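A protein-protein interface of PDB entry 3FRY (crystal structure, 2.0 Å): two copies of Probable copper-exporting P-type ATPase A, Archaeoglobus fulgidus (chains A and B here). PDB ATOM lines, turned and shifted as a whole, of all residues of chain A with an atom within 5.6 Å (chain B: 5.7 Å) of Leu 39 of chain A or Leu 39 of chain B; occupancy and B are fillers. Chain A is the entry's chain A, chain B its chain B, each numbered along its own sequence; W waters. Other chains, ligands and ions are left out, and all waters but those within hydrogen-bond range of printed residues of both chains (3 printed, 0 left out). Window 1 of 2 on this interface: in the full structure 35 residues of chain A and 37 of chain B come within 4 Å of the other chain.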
ATOM      1  N   LEU A  11      26.848  -2.290  10.003  1.00  0.00           N
ATOM      2  CA  LEU A  11      26.032  -2.573  11.181  1.00  0.00           C
ATOM      3  C   LEU A  11      24.543  -2.314  10.957  1.00  0.00           C
ATOM      4  O   LEU A  11      24.164  -1.552  10.075  1.00  0.00           O
ATOM      5  CB  LEU A  11      26.494  -1.713  12.362  1.00  0.00           C
ATOM      6  CG  LEU A  11      27.977  -1.711  12.750  1.00  0.00           C
ATOM      7  CD1 LEU A  11      28.187  -0.750  13.909  1.00  0.00           C
ATOM      8  CD2 LEU A  11      28.422  -3.115  13.136  1.00  0.00           C
ATOM      9  N   SER A  12      23.714  -2.968  11.767  1.00  0.00           N
ATOM     10  CA  SER A  12      22.266  -2.784  11.735  1.00  0.00           C
ATOM     11  C   SER A  12      21.747  -3.099  13.137  1.00  0.00           C
ATOM     12  O   SER A  12      22.380  -3.852  13.889  1.00  0.00           O
ATOM     13  CB  SER A  12      21.603  -3.699  10.698  1.00  0.00           C
ATOM     14  OG  SER A  12      21.751  -5.060  11.039  1.00  0.00           O
ATOM     15  N   LEU A  14      20.714  -0.425  15.134  1.00  0.00           N
ATOM     16  CA  LEU A  14      20.980   0.784  15.919  1.00  0.00           C
ATOM     17  C   LEU A  14      20.094   1.969  15.534  1.00  0.00           C
ATOM     18  O   LEU A  14      20.148   3.025  16.164  1.00  0.00           O
ATOM     19  CB  LEU A  14      22.449   1.210  15.767  1.00  0.00           C
ATOM     20  CG  LEU A  14      23.599   0.275  16.171  1.00  0.00           C
ATOM     21  CD1 LEU A  14      23.515  -0.015  17.644  1.00  0.00           C
ATOM     22  CD2 LEU A  14      23.544  -1.014  15.379  1.00  0.00           C
ATOM     23  N   SER A  15      19.278   1.798  14.503  1.00  0.00           N
ATOM     24  CA  SER A  15      18.434   2.893  14.056  1.00  0.00           C
ATOM     25  C   SER A  15      17.006   2.487  13.753  1.00  0.00           C
ATOM     26  O   SER A  15      16.701   1.306  13.543  1.00  0.00           O
ATOM     27  CB  SER A  15      19.058   3.533  12.819  1.00  0.00           C
ATOM     28  OG  SER A  15      19.415   2.531  11.889  1.00  0.00           O
ATOM     29  N   CYS A  16      16.129   3.483  13.735  1.00  0.00           N
ATOM     30  CA  CYS A  16      14.736   3.242  13.448  1.00  0.00           C
ATOM     31  C   CYS A  16      14.167   4.243  12.456  1.00  0.00           C
ATOM     32  O   CYS A  16      13.464   5.182  12.838  1.00  0.00           O
ATOM     33  CB  CYS A  16      13.897   3.267  14.729  1.00  0.00           C
ATOM     34  SG  CYS A  16      12.211   2.730  14.330  1.00  0.00           S
ATOM     35  N   HIS A  17      14.473   4.045  11.177  1.00  0.00           N
ATOM     36  CA  HIS A  17      13.946   4.932  10.156  1.00  0.00           C
ATOM     37  C   HIS A  17      12.444   4.741  10.000  1.00  0.00           C
ATOM     38  O   HIS A  17      11.739   5.681   9.635  1.00  0.00           O
ATOM     39  CB  HIS A  17      14.640   4.691   8.809  1.00  0.00           C
ATOM     40  CG  HIS A  17      15.944   5.411   8.669  1.00  0.00           C
ATOM     41  ND1 HIS A  17      17.161   4.806   8.898  1.00  0.00           N
ATOM     42  CD2 HIS A  17      16.219   6.703   8.370  1.00  0.00           C
ATOM     43  CE1 HIS A  17      18.128   5.693   8.749  1.00  0.00           C
ATOM     44  NE2 HIS A  17      17.583   6.852   8.428  1.00  0.00           N
ATOM     45  N   VAL A  20      10.166   7.263  11.797  1.00  0.00           N
ATOM     46  CA  VAL A  20      10.013   8.636  11.323  1.00  0.00           C
ATOM     47  C   VAL A  20       8.618   9.094  10.904  1.00  0.00           C
ATOM     48  O   VAL A  20       8.209  10.215  11.222  1.00  0.00           O
ATOM     49  CB  VAL A  20      10.989   8.909  10.152  1.00  0.00           C
ATOM     50  CG1 VAL A  20      10.777  10.304   9.588  1.00  0.00           C
ATOM     51  CG2 VAL A  20      12.411   8.758  10.640  1.00  0.00           C
ATOM     52  N   VAL A  37      12.222  15.824   8.613  1.00  0.00           N
ATOM     53  CA  VAL A  37      12.363  14.987   9.792  1.00  0.00           C
ATOM     54  C   VAL A  37      13.277  13.821   9.449  1.00  0.00           C
ATOM     55  O   VAL A  37      13.127  13.192   8.401  1.00  0.00           O
ATOM     56  CB  VAL A  37      11.001  14.435  10.283  1.00  0.00           C
ATOM     57  CG1 VAL A  37      10.341  13.610   9.185  1.00  0.00           C
ATOM     58  CG2 VAL A  37      11.207  13.583  11.537  1.00  0.00           C
ATOM     59  N   ASP A  38      14.253  13.574  10.319  1.00  0.00           N
ATOM     60  CA  ASP A  38      15.181  12.458  10.169  1.00  0.00           C
ATOM     61  C   ASP A  38      15.411  11.878  11.561  1.00  0.00           C
ATOM     62  O   ASP A  38      14.688  12.225  12.501  1.00  0.00           O
ATOM     63  CB  ASP A  38      16.516  12.881   9.523  1.00  0.00           C
ATOM     64  CG  ASP A  38      17.187  14.049  10.232  1.00  0.00           C
ATOM     65  OD1 ASP A  38      17.151  14.121  11.479  1.00  0.00           O
ATOM     66  OD2 ASP A  38      17.773  14.895   9.523  1.00  0.00           O
ATOM     67  N   LEU A  39      16.408  11.014  11.709  1.00  0.00           N
ATOM     68  CA  LEU A  39      16.662  10.383  13.006  1.00  0.00           C
ATOM     69  C   LEU A  39      16.976  11.327  14.169  1.00  0.00           C
ATOM     70  O   LEU A  39      16.613  11.051  15.318  1.00  0.00           O
ATOM     71  CB  LEU A  39      17.807   9.374  12.888  1.00  0.00           C
ATOM     72  CG  LEU A  39      17.656   8.216  11.896  1.00  0.00           C
ATOM     73  CD1 LEU A  39      18.877   7.307  12.005  1.00  0.00           C
ATOM     74  CD2 LEU A  39      16.381   7.435  12.191  1.00  0.00           C
ATOM     75  N   ASN A  40      17.640  12.438  13.873  1.00  0.00           N
ATOM     76  CA  ASN A  40      18.051  13.368  14.915  1.00  0.00           C
ATOM     77  C   ASN A  40      17.279  14.661  15.071  1.00  0.00           C
ATOM     78  O   ASN A  40      17.412  15.330  16.093  1.00  0.00           O
ATOM     79  CB  ASN A  40      19.525  13.719  14.721  1.00  0.00           C
ATOM     80  CG  ASN A  40      20.391  12.496  14.609  1.00  0.00           C
ATOM     81  OD1 ASN A  40      20.347  11.619  15.472  1.00  0.00           O
ATOM     82  ND2 ASN A  40      21.183  12.421  13.546  1.00  0.00           N
ATOM     83  N   GLU A  41      16.482  15.029  14.078  1.00  0.00           N
ATOM     84  CA  GLU A  41      15.765  16.287  14.185  1.00  0.00           C
ATOM     85  C   GLU A  41      14.504  16.391  13.360  1.00  0.00           C
ATOM     86  O   GLU A  41      14.304  15.669  12.384  1.00  0.00           O
ATOM     87  CB  GLU A  41      16.684  17.451  13.786  1.00  0.00           C
ATOM     88  CG  GLU A  41      17.294  17.292  12.395  1.00  0.00           C
ATOM     89  CD  GLU A  41      17.859  18.588  11.819  1.00  0.00           C
ATOM     90  OE1 GLU A  41      18.448  19.388  12.578  1.00  0.00           O
ATOM     91  OE2 GLU A  41      17.728  18.795  10.594  1.00  0.00           O
ATOM     92  N   LEU B  11      15.676  15.322  18.198  1.00  0.00           N
ATOM     93  CA  LEU B  11      14.994  14.085  18.552  1.00  0.00           C
ATOM     94  C   LEU B  11      15.891  13.029  19.192  1.00  0.00           C
ATOM     95  O   LEU B  11      17.094  12.972  18.932  1.00  0.00           O
ATOM     96  CB  LEU B  11      14.339  13.487  17.302  1.00  0.00           C
ATOM     97  CG  LEU B  11      13.454  14.430  16.476  1.00  0.00           C
ATOM     98  CD1 LEU B  11      12.983  13.733  15.217  1.00  0.00           C
ATOM     99  CD2 LEU B  11      12.267  14.875  17.324  1.00  0.00           C
ATOM    100  N   SER B  12      15.278  12.194  20.025  1.00  0.00           N
ATOM    101  CA  SER B  12      15.968  11.093  20.692  1.00  0.00           C
ATOM    102  C   SER B  12      15.029   9.891  20.645  1.00  0.00           C
ATOM    103  O   SER B  12      13.812  10.049  20.709  1.00  0.00           O
ATOM    104  CB  SER B  12      16.274  11.448  22.154  1.00  0.00           C
ATOM    105  OG  SER B  12      17.160  12.550  22.241  1.00  0.00           O
ATOM    106  N   LEU B  14      14.968   7.546  18.049  1.00  0.00           N
ATOM    107  CA  LEU B  14      14.820   6.977  16.706  1.00  0.00           C
ATOM    108  C   LEU B  14      16.115   6.296  16.282  1.00  0.00           C
ATOM    109  O   LEU B  14      16.198   5.681  15.218  1.00  0.00           O
ATOM    110  CB  LEU B  14      14.446   8.043  15.677  1.00  0.00           C
ATOM    111  CG  LEU B  14      13.007   8.559  15.745  1.00  0.00           C
ATOM    112  CD1 LEU B  14      12.895   9.640  16.827  1.00  0.00           C
ATOM    113  CD2 LEU B  14      12.611   9.133  14.383  1.00  0.00           C
ATOM    114  N   SER B  15      17.129   6.421  17.127  1.00  0.00           N
ATOM    115  CA  SER B  15      18.427   5.802  16.895  1.00  0.00           C
ATOM    116  C   SER B  15      19.032   5.646  18.280  1.00  0.00           C
ATOM    117  O   SER B  15      18.663   6.375  19.205  1.00  0.00           O
ATOM    118  CB  SER B  15      19.313   6.694  16.020  1.00  0.00           C
ATOM    119  OG  SER B  15      19.701   7.857  16.714  1.00  0.00           O
ATOM    120  N   CYS B  16      19.956   4.704  18.433  1.00  0.00           N
ATOM    121  CA  CYS B  16      20.559   4.465  19.734  1.00  0.00           C
ATOM    122  C   CYS B  16      22.063   4.710  19.739  1.00  0.00           C
ATOM    123  O   CYS B  16      22.847   3.841  19.352  1.00  0.00           O
ATOM    124  CB  CYS B  16      20.242   3.033  20.187  1.00  0.00           C
ATOM    125  SG  CYS B  16      20.998   2.565  21.774  1.00  0.00           S
ATOM    126  N   HIS B  17      22.462   5.898  20.183  1.00  0.00           N
ATOM    127  CA  HIS B  17      23.875   6.237  20.228  1.00  0.00           C
ATOM    128  C   HIS B  17      24.613   5.545  21.371  1.00  0.00           C
ATOM    129  O   HIS B  17      25.824   5.361  21.291  1.00  0.00           O
ATOM    130  CB  HIS B  17      24.070   7.759  20.300  1.00  0.00           C
ATOM    131  CG  HIS B  17      23.722   8.467  19.025  1.00  0.00           C
ATOM    132  ND1 HIS B  17      22.426   8.794  18.683  1.00  0.00           N
ATOM    133  CD2 HIS B  17      24.493   8.849  17.979  1.00  0.00           C
ATOM    134  CE1 HIS B  17      22.414   9.343  17.481  1.00  0.00           C
ATOM    135  NE2 HIS B  17      23.655   9.386  17.031  1.00  0.00           N
ATOM    136  N   VAL B  20      26.074   2.432  20.263  1.00  0.00           N
ATOM    137  CA  VAL B  20      27.302   2.577  19.492  1.00  0.00           C
ATOM    138  C   VAL B  20      28.495   2.294  20.399  1.00  0.00           C
ATOM    139  O   VAL B  20      29.426   1.590  20.009  1.00  0.00           O
ATOM    140  CB  VAL B  20      27.431   3.994  18.901  1.00  0.00           C
ATOM    141  CG1 VAL B  20      28.829   4.198  18.315  1.00  0.00           C
ATOM    142  CG2 VAL B  20      26.376   4.189  17.818  1.00  0.00           C
ATOM    143  N   VAL B  37      33.081   4.250  14.528  1.00  0.00           N
ATOM    144  CA  VAL B  37      31.876   3.463  14.673  1.00  0.00           C
ATOM    145  C   VAL B  37      30.672   4.377  14.840  1.00  0.00           C
ATOM    146  O   VAL B  37      30.650   5.242  15.711  1.00  0.00           O
ATOM    147  CB  VAL B  37      31.982   2.503  15.887  1.00  0.00           C
ATOM    148  CG1 VAL B  37      32.282   3.292  17.155  1.00  0.00           C
ATOM    149  CG2 VAL B  37      30.688   1.704  16.036  1.00  0.00           C
ATOM    150  N   ASP B  38      29.682   4.196  13.976  1.00  0.00           N
ATOM    151  CA  ASP B  38      28.464   4.985  14.045  1.00  0.00           C
ATOM    152  C   ASP B  38      27.282   4.035  13.960  1.00  0.00           C
ATOM    153  O   ASP B  38      27.427   2.838  14.204  1.00  0.00           O
ATOM    154  CB  ASP B  38      28.404   6.015  12.911  1.00  0.00           C
ATOM    155  CG  ASP B  38      28.584   5.398  11.537  1.00  0.00           C
ATOM    156  OD1 ASP B  38      28.027   4.310  11.275  1.00  0.00           O
ATOM    157  OD2 ASP B  38      29.275   6.021  10.702  1.00  0.00           O
ATOM    158  N   LEU B  39      26.118   4.564  13.601  1.00  0.00           N
ATOM    159  CA  LEU B  39      24.915   3.746  13.506  1.00  0.00           C
ATOM    160  C   LEU B  39      24.975   2.686  12.415  1.00  0.00           C
ATOM    161  O   LEU B  39      24.413   1.606  12.568  1.00  0.00           O
ATOM    162  CB  LEU B  39      23.690   4.629  13.239  1.00  0.00           C
ATOM    163  CG  LEU B  39      23.372   5.765  14.208  1.00  0.00           C
ATOM    164  CD1 LEU B  39      22.154   6.515  13.684  1.00  0.00           C
ATOM    165  CD2 LEU B  39      23.109   5.214  15.605  1.00  0.00           C
ATOM    166  N   ASN B  40      25.668   2.986  11.322  1.00  0.00           N
ATOM    167  CA  ASN B  40      25.715   2.057  10.198  1.00  0.00           C
ATOM    168  C   ASN B  40      26.981   1.260   9.923  1.00  0.00           C
ATOM    169  O   ASN B  40      26.964   0.360   9.088  1.00  0.00           O
ATOM    170  CB  ASN B  40      25.322   2.805   8.931  1.00  0.00           C
ATOM    171  CG  ASN B  40      23.985   3.507   9.077  1.00  0.00           C
ATOM    172  OD1 ASN B  40      22.963   2.865   9.327  1.00  0.00           O
ATOM    173  ND2 ASN B  40      23.989   4.829   8.933  1.00  0.00           N
ATOM    174  N   GLU B  41      28.075   1.580  10.597  1.00  0.00           N
ATOM    175  CA  GLU B  41      29.307   0.844  10.361  1.00  0.00           C
ATOM    176  C   GLU B  41      30.326   0.962  11.482  1.00  0.00           C
ATOM    177  O   GLU B  41      30.248   1.844  12.339  1.00  0.00           O
ATOM    178  CB  GLU B  41      29.965   1.301   9.049  1.00  0.00           C
ATOM    179  CG  GLU B  41      30.194   2.798   8.953  1.00  0.00           C
ATOM    180  CD  GLU B  41      31.193   3.185   7.865  1.00  0.00           C
ATOM    181  OE1 GLU B  41      31.170   2.569   6.775  1.00  0.00           O
ATOM    182  OE2 GLU B  41      31.992   4.123   8.104  1.00  0.00           O
HETATM  183  O   HOH W   1      22.402   0.271   9.370  1.00  0.00           O
HETATM  184  O   HOH W   2      21.691   0.500  12.700  1.00  0.00           O
HETATM  185  O   HOH W   3      16.560   9.922  17.604  1.00  0.00           O
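The backbone carbonyl oxygen of Asn 40 of chain B is in hydrogen-bond range of the backbone NH of Leu 11 of chain A. N of Cys 16 of chain B is in hydrogen-bond range of O of Leu 14 of chain A (2.8 Å). The backbone NH (N) of Cys 16 of chain A is in hydrogen-bond range of the backbone carbonyl oxygen (O) of Leu 14 of chain B (2.7 Å). The backbone carbonyl oxygen (O) of Asn 40 of chain A sits at hydrogen-bond distance from the backbone NH (N) of Leu 11 of chain B.
The side-chain carboxylate of Asp 38 of chain B lies within hydrogen-bond range of the backbone NH of Glu 41 of chain B (2.8 Å). The side-chain carboxylate of Asp 38 of chain A sits at hydrogen-bond distance from the backbone NH of Asn 40 of chain A (3.0 Å). N of Asn 40 of chain B sits at hydrogen-bond distance from OD1 of Asp 38 of chain B (2.7 Å). The side-chain carboxylate of Asp 38 of chain A sits at hydrogen-bond distance from the backbone NH of Glu 41 of chain A, at 2.8 Å. The side-chain hydroxyl of Ser 15 of chain B sits close to a ring nitrogen (ND1) of His 17 of chain B (3.5 Å).
Among the printed residues, pairs that only touch across the chains: Leu 11 of chain A with Asp 38 of chain B, Leu 11 of chain A with Leu 39 of chain B, Leu 11 of chain A with Glu 41 of chain B, Leu 14 of chain A with Ser 15 of chain B, Leu 14 of chain A with Leu 39 of chain B, Ser 15 of chain A with Leu 14 of chain B, Val 20 of chain A with Leu 14 of chain B, Asp 38 of chain A with Leu 11 of chain B, Leu 39 of chain A with Leu 11 of chain B, Leu 39 of chain A with Leu 14 of chain B, Leu 39 of chain A with Leu 39 of chain B, Asn 40 of chain A with His 17 of chain B and Glu 41 of chain A with Leu 11 of chain B.
Of chain B, only Leu 11 (3.9 Å), Leu 14 (3.5 Å) and Leu 39 (3.8 Å) come within 4 Å of Leu 39 of chain A. Of the printed residues of chain A, Leu 11 of chain B touches Asp 38, Leu 39, Asn 40 and Glu 41. Val 20 of chain B touches none of the printed residues of chain A. Val 37 of chain B touches none of the printed residues of chain A. Of the printed residues of chain A, Asp 38 of chain B touches Leu 11 (3.7 Å). Leu 39 of chain B touches just these residues of chain A: Leu 11, Leu 14 and Leu 39. The nearest residue of chain A that does not touch Leu 39 of chain B is Ser 15 of chain A (4.4 Å).
Of the 12 printed residues of chain B, 9 touch a printed residue of chain A. Printed residues of chain B that touch a printed residue of chain A: Leu 11, Leu 14, Ser 15, Cys 16, His 17, Asp 38, Leu 39, Asn 40 and Glu 41. Hydrophobic or aromatic side chains of chain B that line the printed part of chain A: Leu 11, Leu 14, His 17 and Leu 39. Of the 12 printed residues of chain A, 9 touch a printed residue of chain B. Among the printed residues, 17 pairs touch across the chains. Among the printed residues, no Asp or Glu carboxylate lies within 4 Å of a Lys or Arg side-chain nitrogen of the other chain.
Leu 11 of chain A touches Asn 40 of chain B, and with the chains exchanged Asn 40 of chain A touches Leu 11 of chain B. Leu 14 of chain A touches Cys 16 of chain B, and with the chains exchanged Cys 16 of chain A touches Leu 14 of chain B. Leu 14 of chain A touches Leu 39 of chain B, and with the chains exchanged Leu 39 of chain A touches Leu 14 of chain B. Asn 40 of chain A touches His 17 of chain B, but with the chains exchanged His 17 of chain A does not touch Asn 40 of chain B (5.6 Å).
Water W3 lies within hydrogen-bond range of O of Leu 39 of chain A, N of Leu 14 of chain B and O of Leu 11 of chain B. Water W1 bridges O of Leu 11 of chain A and OD1 of Asn 40 of chain B. Water W2 lies within hydrogen-bond range of the backbone NH (N) of Leu 14 of chain A, the backbone carbonyl oxygen (O) of Leu 39 of chain B and the side-chain hydroxyl (OG) of Ser 15 of chain A.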
